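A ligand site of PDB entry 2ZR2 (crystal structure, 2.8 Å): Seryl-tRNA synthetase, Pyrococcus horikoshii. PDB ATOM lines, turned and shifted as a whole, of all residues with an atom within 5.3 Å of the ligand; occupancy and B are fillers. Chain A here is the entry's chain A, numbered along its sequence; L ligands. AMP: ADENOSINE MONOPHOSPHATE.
O of Phe 297 lies close to N1 of the ligand (3.2 Å). Arg 298 touches the ligand. Phe 302 touches the ligand. Lys 304 touches the ligand. Val 372 touches the ligand. CB of Ser 373 touches O1P of the ligand, 3.6 Å away. Thr 406 touches the ligand. Ala 409 touches the ligand. Arg 412 touches the ligand (CD to C2', 3.5 Å). Hydrophobic or aromatic side chains within 4 Å of the ligand: Val 299, Phe 302 and Ala 409. 15 residues have an atom within 4 Å of the ligand: Arg 283, Glu 285, Phe 297, Arg 298, Val 299, Phe 302, Lys 304, Glu 370, Val 371, Val 372, Ser 373, Thr 406, Ala 409, Ser 411 and Arg 412. The nearest printed residue that does not touch the ligand is Ile 296 (4.3 Å).
An oxygen (O3') of the ligand is in hydrogen-bond range of the side-chain carboxylate (OE1) of Glu 370. NH2 of Arg 283 lies within salt-bridge range of O3P of the ligand (2.8 Å). O of Val 371 is in hydrogen-bond range of O2' of the ligand. A nitrogen (N6) of the ligand sits at hydrogen-bond distance from the side-chain carboxylate of Glu 285. A nitrogen (N1) of the ligand is in hydrogen-bond range of the backbone NH of Val 299 (3.1 Å). The backbone carbonyl oxygen (O) of Val 299 lies within hydrogen-bond range of a nitrogen (N6) of the ligand (3.1 Å). A nitrogen (N3) of the ligand sits at hydrogen-bond distance from the side-chain hydroxyl (OG) of Ser 411 (3.1 Å).
The backbone carbonyl oxygen (O) of Glu 370 lies within hydrogen-bond range of the guanidinium group (NH2) of Arg 412. NH1 of Arg 283 sits at hydrogen-bond distance from O of Pro 251 (2.9 Å). The backbone carbonyl oxygen (O) of Arg 283 sits at hydrogen-bond distance from a ring nitrogen (ND1) of His 300 (2.8 Å). The backbone carbonyl oxygen (O) of Phe 297 sits at hydrogen-bond distance from the guanidinium group (NE) of Arg 412, 2.8 Å away. N of Ser 373 lies within hydrogen-bond range of OG1 of Thr 406 (3.1 Å). The side-chain amino group of Lys 304 is in hydrogen-bond range of the side-chain hydroxyl of Thr 252.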
ATOM      1  N   PRO A 251     -25.013  -0.571  14.106  1.00  0.00           N
ATOM      2  CA  PRO A 251     -24.598  -0.490  15.500  1.00  0.00           C
ATOM      3  C   PRO A 251     -23.899   0.830  15.793  1.00  0.00           C
ATOM      4  O   PRO A 251     -23.593   1.152  16.945  1.00  0.00           O
ATOM      5  CB  PRO A 251     -23.658  -1.671  15.645  1.00  0.00           C
ATOM      6  CG  PRO A 251     -23.018  -1.737  14.292  1.00  0.00           C
ATOM      7  CD  PRO A 251     -24.181  -1.539  13.360  1.00  0.00           C
ATOM      8  N   THR A 252     -23.656   1.592  14.731  1.00  0.00           N
ATOM      9  CA  THR A 252     -22.986   2.879  14.798  1.00  0.00           C
ATOM     10  C   THR A 252     -23.028   3.536  13.413  1.00  0.00           C
ATOM     11  O   THR A 252     -23.018   2.841  12.407  1.00  0.00           O
ATOM     12  CB  THR A 252     -21.507   2.687  15.232  1.00  0.00           C
ATOM     13  OG1 THR A 252     -20.750   3.846  14.889  1.00  0.00           O
ATOM     14  CG2 THR A 252     -20.902   1.457  14.572  1.00  0.00           C
ATOM     15  N   GLU A 254     -20.807   4.924  12.046  1.00  0.00           N
ATOM     16  CA  GLU A 254     -19.511   4.617  11.467  1.00  0.00           C
ATOM     17  C   GLU A 254     -19.673   3.752  10.220  1.00  0.00           C
ATOM     18  O   GLU A 254     -19.131   4.054   9.158  1.00  0.00           O
ATOM     19  CB  GLU A 254     -18.645   3.863  12.486  1.00  0.00           C
ATOM     20  CG  GLU A 254     -17.308   3.370  11.971  1.00  0.00           C
ATOM     21  CD  GLU A 254     -16.672   2.314  12.866  1.00  0.00           C
ATOM     22  OE1 GLU A 254     -16.867   2.425  14.102  1.00  0.00           O
ATOM     23  OE2 GLU A 254     -15.986   1.390  12.346  1.00  0.00           O
ATOM     24  N   ARG A 283     -27.547  -2.571  19.261  1.00  0.00           N
ATOM     25  CA  ARG A 283     -26.589  -3.622  19.608  1.00  0.00           C
ATOM     26  C   ARG A 283     -27.267  -4.724  20.395  1.00  0.00           C
ATOM     27  O   ARG A 283     -28.054  -4.462  21.314  1.00  0.00           O
ATOM     28  CB  ARG A 283     -25.459  -3.045  20.464  1.00  0.00           C
ATOM     29  CG  ARG A 283     -25.230  -1.568  20.291  1.00  0.00           C
ATOM     30  CD  ARG A 283     -24.108  -1.226  19.348  1.00  0.00           C
ATOM     31  NE  ARG A 283     -22.823  -1.468  19.992  1.00  0.00           N
ATOM     32  CZ  ARG A 283     -21.770  -0.653  19.887  1.00  0.00           C
ATOM     33  NH1 ARG A 283     -21.848   0.460  19.163  1.00  0.00           N
ATOM     34  NH2 ARG A 283     -20.646  -0.969  20.496  1.00  0.00           N
ATOM     35  N   GLU A 285     -25.636  -6.863  22.253  1.00  0.00           N
ATOM     36  CA  GLU A 285     -24.954  -6.964  23.537  1.00  0.00           C
ATOM     37  C   GLU A 285     -25.104  -8.393  24.047  1.00  0.00           C
ATOM     38  O   GLU A 285     -25.276  -8.612  25.244  1.00  0.00           O
ATOM     39  CB  GLU A 285     -25.552  -5.992  24.558  1.00  0.00           C
ATOM     40  CG  GLU A 285     -25.127  -4.535  24.380  1.00  0.00           C
ATOM     41  CD  GLU A 285     -23.610  -4.361  24.367  1.00  0.00           C
ATOM     42  OE1 GLU A 285     -22.901  -5.152  25.017  1.00  0.00           O
ATOM     43  OE2 GLU A 285     -23.125  -3.410  23.703  1.00  0.00           O
ATOM     44  N   ILE A 296     -28.948   3.075  31.754  1.00  0.00           N
ATOM     45  CA  ILE A 296     -28.700   3.339  30.329  1.00  0.00           C
ATOM     46  C   ILE A 296     -27.227   3.364  29.929  1.00  0.00           C
ATOM     47  O   ILE A 296     -26.848   4.025  28.963  1.00  0.00           O
ATOM     48  CB  ILE A 296     -29.319   4.684  29.905  1.00  0.00           C
ATOM     49  CG1 ILE A 296     -28.719   5.813  30.740  1.00  0.00           C
ATOM     50  CG2 ILE A 296     -30.839   4.605  30.034  1.00  0.00           C
ATOM     51  CD1 ILE A 296     -29.245   7.242  30.386  1.00  0.00           C
ATOM     52  N   PHE A 297     -26.391   2.651  30.678  1.00  0.00           N
ATOM     53  CA  PHE A 297     -24.959   2.608  30.381  1.00  0.00           C
ATOM     54  C   PHE A 297     -24.671   1.633  29.250  1.00  0.00           C
ATOM     55  O   PHE A 297     -23.907   1.939  28.337  1.00  0.00           O
ATOM     56  CB  PHE A 297     -24.162   2.171  31.601  1.00  0.00           C
ATOM     57  CG  PHE A 297     -22.681   2.224  31.380  1.00  0.00           C
ATOM     58  CD1 PHE A 297     -22.034   3.456  31.239  1.00  0.00           C
ATOM     59  CD2 PHE A 297     -21.945   1.044  31.269  1.00  0.00           C
ATOM     60  CE1 PHE A 297     -20.654   3.512  30.970  1.00  0.00           C
ATOM     61  CE2 PHE A 297     -20.562   1.089  31.008  1.00  0.00           C
ATOM     62  CZ  PHE A 297     -19.912   2.338  30.853  1.00  0.00           C
ATOM     63  N   ARG A 298     -25.268   0.447  29.329  1.00  0.00           N
ATOM     64  CA  ARG A 298     -25.071  -0.584  28.320  1.00  0.00           C
ATOM     65  C   ARG A 298     -26.452  -1.101  27.921  1.00  0.00           C
ATOM     66  O   ARG A 298     -26.969  -2.040  28.527  1.00  0.00           O
ATOM     67  CB  ARG A 298     -24.202  -1.717  28.873  1.00  0.00           C
ATOM     68  CG  ARG A 298     -23.988  -2.834  27.854  1.00  0.00           C
ATOM     69  CD  ARG A 298     -23.180  -4.005  28.388  1.00  0.00           C
ATOM     70  NE  ARG A 298     -21.785  -3.654  28.636  1.00  0.00           N
ATOM     71  CZ  ARG A 298     -21.320  -3.269  29.808  1.00  0.00           C
ATOM     72  NH1 ARG A 298     -22.125  -3.204  30.866  1.00  0.00           N
ATOM     73  NH2 ARG A 298     -20.042  -2.937  29.924  1.00  0.00           N
ATOM     74  N   VAL A 299     -27.026  -0.500  26.893  1.00  0.00           N
ATOM     75  CA  VAL A 299     -28.359  -0.872  26.456  1.00  0.00           C
ATOM     76  C   VAL A 299     -28.404  -1.324  25.002  1.00  0.00           C
ATOM     77  O   VAL A 299     -27.398  -1.300  24.307  1.00  0.00           O
ATOM     78  CB  VAL A 299     -29.305   0.317  26.621  1.00  0.00           C
ATOM     79  CG1 VAL A 299     -29.509   0.631  28.080  1.00  0.00           C
ATOM     80  CG2 VAL A 299     -28.684   1.548  25.951  1.00  0.00           C
ATOM     81  N   HIS A 300     -29.577  -1.720  24.552  1.00  0.00           N
ATOM     82  CA  HIS A 300     -29.744  -2.146  23.171  1.00  0.00           C
ATOM     83  C   HIS A 300     -29.788  -0.996  22.164  1.00  0.00           C
ATOM     84  O   HIS A 300     -29.399  -1.184  21.004  1.00  0.00           O
ATOM     85  CB  HIS A 300     -30.989  -3.017  23.037  1.00  0.00           C
ATOM     86  CG  HIS A 300     -30.845  -4.344  23.683  1.00  0.00           C
ATOM     87  ND1 HIS A 300     -29.842  -5.226  23.343  1.00  0.00           N
ATOM     88  CD2 HIS A 300     -31.560  -4.944  24.668  1.00  0.00           C
ATOM     89  CE1 HIS A 300     -29.952  -6.323  24.077  1.00  0.00           C
ATOM     90  NE2 HIS A 300     -30.978  -6.172  24.889  1.00  0.00           N
ATOM     91  N   PHE A 302     -29.061   3.404  21.555  1.00  0.00           N
ATOM     92  CA  PHE A 302     -28.570   4.695  22.031  1.00  0.00           C
ATOM     93  C   PHE A 302     -28.274   5.578  20.848  1.00  0.00           C
ATOM     94  O   PHE A 302     -28.108   5.105  19.728  1.00  0.00           O
ATOM     95  CB  PHE A 302     -27.310   4.561  22.897  1.00  0.00           C
ATOM     96  CG  PHE A 302     -26.195   3.790  22.240  1.00  0.00           C
ATOM     97  CD1 PHE A 302     -26.244   2.406  22.144  1.00  0.00           C
ATOM     98  CD2 PHE A 302     -25.078   4.452  21.745  1.00  0.00           C
ATOM     99  CE1 PHE A 302     -25.199   1.686  21.552  1.00  0.00           C
ATOM    100  CE2 PHE A 302     -24.021   3.745  21.142  1.00  0.00           C
ATOM    101  CZ  PHE A 302     -24.084   2.359  21.048  1.00  0.00           C
ATOM    102  N   LYS A 304     -25.845   8.390  18.972  1.00  0.00           N
ATOM    103  CA  LYS A 304     -24.438   8.712  18.926  1.00  0.00           C
ATOM    104  C   LYS A 304     -24.015   9.554  17.732  1.00  0.00           C
ATOM    105  O   LYS A 304     -24.334   9.236  16.590  1.00  0.00           O
ATOM    106  CB  LYS A 304     -23.595   7.446  18.977  1.00  0.00           C
ATOM    107  CG  LYS A 304     -22.091   7.733  18.878  1.00  0.00           C
ATOM    108  CD  LYS A 304     -21.225   6.525  19.237  1.00  0.00           C
ATOM    109  CE  LYS A 304     -21.463   5.354  18.279  1.00  0.00           C
ATOM    110  NZ  LYS A 304     -21.412   5.814  16.865  1.00  0.00           N
ATOM    111  N   GLU A 370     -15.604   3.798  29.980  1.00  0.00           N
ATOM    112  CA  GLU A 370     -15.485   4.273  28.601  1.00  0.00           C
ATOM    113  C   GLU A 370     -16.660   5.137  28.231  1.00  0.00           C
ATOM    114  O   GLU A 370     -17.813   4.821  28.538  1.00  0.00           O
ATOM    115  CB  GLU A 370     -15.413   3.121  27.616  1.00  0.00           C
ATOM    116  CG  GLU A 370     -15.431   3.587  26.174  1.00  0.00           C
ATOM    117  CD  GLU A 370     -15.564   2.454  25.183  1.00  0.00           C
ATOM    118  OE1 GLU A 370     -15.831   2.730  23.986  1.00  0.00           O
ATOM    119  OE2 GLU A 370     -15.414   1.285  25.607  1.00  0.00           O
ATOM    120  N   VAL A 371     -16.360   6.226  27.559  1.00  0.00           N
ATOM    121  CA  VAL A 371     -17.388   7.132  27.149  1.00  0.00           C
ATOM    122  C   VAL A 371     -17.189   7.469  25.646  1.00  0.00           C
ATOM    123  O   VAL A 371     -18.133   7.860  24.960  1.00  0.00           O
ATOM    124  CB  VAL A 371     -17.360   8.343  28.085  1.00  0.00           C
ATOM    125  CG1 VAL A 371     -16.510   9.462  27.504  1.00  0.00           C
ATOM    126  CG2 VAL A 371     -18.761   8.758  28.435  1.00  0.00           C
ATOM    127  N   VAL A 372     -15.977   7.309  25.121  1.00  0.00           N
ATOM    128  CA  VAL A 372     -15.730   7.520  23.687  1.00  0.00           C
ATOM    129  C   VAL A 372     -14.563   6.669  23.216  1.00  0.00           C
ATOM    130  O   VAL A 372     -13.712   6.274  24.010  1.00  0.00           O
ATOM    131  CB  VAL A 372     -15.449   9.015  23.246  1.00  0.00           C
ATOM    132  CG1 VAL A 372     -15.945   9.978  24.270  1.00  0.00           C
ATOM    133  CG2 VAL A 372     -13.985   9.216  22.938  1.00  0.00           C
ATOM    134  N   SER A 373     -14.529   6.400  21.919  1.00  0.00           N
ATOM    135  CA  SER A 373     -13.432   5.607  21.369  1.00  0.00           C
ATOM    136  C   SER A 373     -13.021   6.092  19.969  1.00  0.00           C
ATOM    137  O   SER A 373     -13.864   6.270  19.089  1.00  0.00           O
ATOM    138  CB  SER A 373     -13.842   4.147  21.347  1.00  0.00           C
ATOM    139  OG  SER A 373     -12.729   3.343  20.993  1.00  0.00           O
ATOM    140  N   THR A 406     -15.988   8.504  18.529  1.00  0.00           N
ATOM    141  CA  THR A 406     -17.210   8.973  19.120  1.00  0.00           C
ATOM    142  C   THR A 406     -17.043  10.479  19.243  1.00  0.00           C
ATOM    143  O   THR A 406     -15.924  10.963  19.301  1.00  0.00           O
ATOM    144  CB  THR A 406     -17.368   8.389  20.534  1.00  0.00           C
ATOM    145  OG1 THR A 406     -17.192   6.977  20.474  1.00  0.00           O
ATOM    146  CG2 THR A 406     -18.730   8.710  21.118  1.00  0.00           C
ATOM    147  N   ALA A 409     -21.957   9.919  22.656  1.00  0.00           N
ATOM    148  CA  ALA A 409     -22.953   8.874  22.595  1.00  0.00           C
ATOM    149  C   ALA A 409     -23.761   9.345  23.808  1.00  0.00           C
ATOM    150  O   ALA A 409     -23.281   9.288  24.928  1.00  0.00           O
ATOM    151  CB  ALA A 409     -22.302   7.529  22.841  1.00  0.00           C
ATOM    152  N   SER A 411     -26.243   8.255  25.627  1.00  0.00           N
ATOM    153  CA  SER A 411     -26.441   7.302  26.733  1.00  0.00           C
ATOM    154  C   SER A 411     -25.402   7.552  27.856  1.00  0.00           C
ATOM    155  O   SER A 411     -25.759   7.970  28.951  1.00  0.00           O
ATOM    156  CB  SER A 411     -26.273   5.883  26.212  1.00  0.00           C
ATOM    157  OG  SER A 411     -25.036   5.797  25.478  1.00  0.00           O
ATOM    158  N   ARG A 412     -24.126   7.314  27.553  1.00  0.00           N
ATOM    159  CA  ARG A 412     -23.088   7.474  28.544  1.00  0.00           C
ATOM    160  C   ARG A 412     -22.753   8.910  28.915  1.00  0.00           C
ATOM    161  O   ARG A 412     -22.412   9.196  30.080  1.00  0.00           O
ATOM    162  CB  ARG A 412     -21.862   6.700  28.098  1.00  0.00           C
ATOM    163  CG  ARG A 412     -22.201   5.240  27.922  1.00  0.00           C
ATOM    164  CD  ARG A 412     -20.993   4.382  27.681  1.00  0.00           C
ATOM    165  NE  ARG A 412     -21.368   2.969  27.698  1.00  0.00           N
ATOM    166  CZ  ARG A 412     -20.515   1.971  27.516  1.00  0.00           C
ATOM    167  NH1 ARG A 412     -20.957   0.706  27.548  1.00  0.00           N
ATOM    168  NH2 ARG A 412     -19.220   2.205  27.317  1.00  0.00           N
HETATM  169  P   AMP L   1     -17.726   1.411  19.825  1.00  0.00           P
HETATM  170  O1P AMP L   1     -16.403   2.067  19.854  1.00  0.00           O
HETATM  171  O2P AMP L   1     -18.789   1.698  18.669  1.00  0.00           O
HETATM  172  O3P AMP L   1     -18.013   0.005  20.601  1.00  0.00           O
HETATM  173  O5' AMP L   1     -18.516   2.295  20.935  1.00  0.00           O
HETATM  174  C5' AMP L   1     -18.285   3.699  21.058  1.00  0.00           C
HETATM  175  C4' AMP L   1     -19.128   4.308  22.155  1.00  0.00           C
HETATM  176  O4' AMP L   1     -20.531   4.014  21.951  1.00  0.00           O
HETATM  177  C3' AMP L   1     -18.817   3.733  23.528  1.00  0.00           C
HETATM  178  O3' AMP L   1     -17.655   4.364  24.064  1.00  0.00           O
HETATM  179  C2' AMP L   1     -20.023   4.226  24.301  1.00  0.00           C
HETATM  180  O2' AMP L   1     -19.900   5.619  24.564  1.00  0.00           O
HETATM  181  C1' AMP L   1     -21.164   3.959  23.297  1.00  0.00           C
HETATM  182  N9  AMP L   1     -21.714   2.584  23.481  1.00  0.00           N
HETATM  183  C8  AMP L   1     -21.237   1.440  22.962  1.00  0.00           C
HETATM  184  N7  AMP L   1     -22.033   0.433  23.316  1.00  0.00           N
HETATM  185  C5  AMP L   1     -23.021   0.926  24.055  1.00  0.00           C
HETATM  186  C6  AMP L   1     -24.126   0.380  24.687  1.00  0.00           C
HETATM  187  N6  AMP L   1     -24.363  -0.919  24.610  1.00  0.00           N
HETATM  188  N1  AMP L   1     -24.972   1.182  25.384  1.00  0.00           N
HETATM  189  C2  AMP L   1     -24.758   2.507  25.468  1.00  0.00           C
HETATM  190  N3  AMP L   1     -23.695   3.059  24.858  1.00  0.00           N
HETATM  191  C4  AMP L   1     -22.816   2.297  24.167  1.00  0.00           C
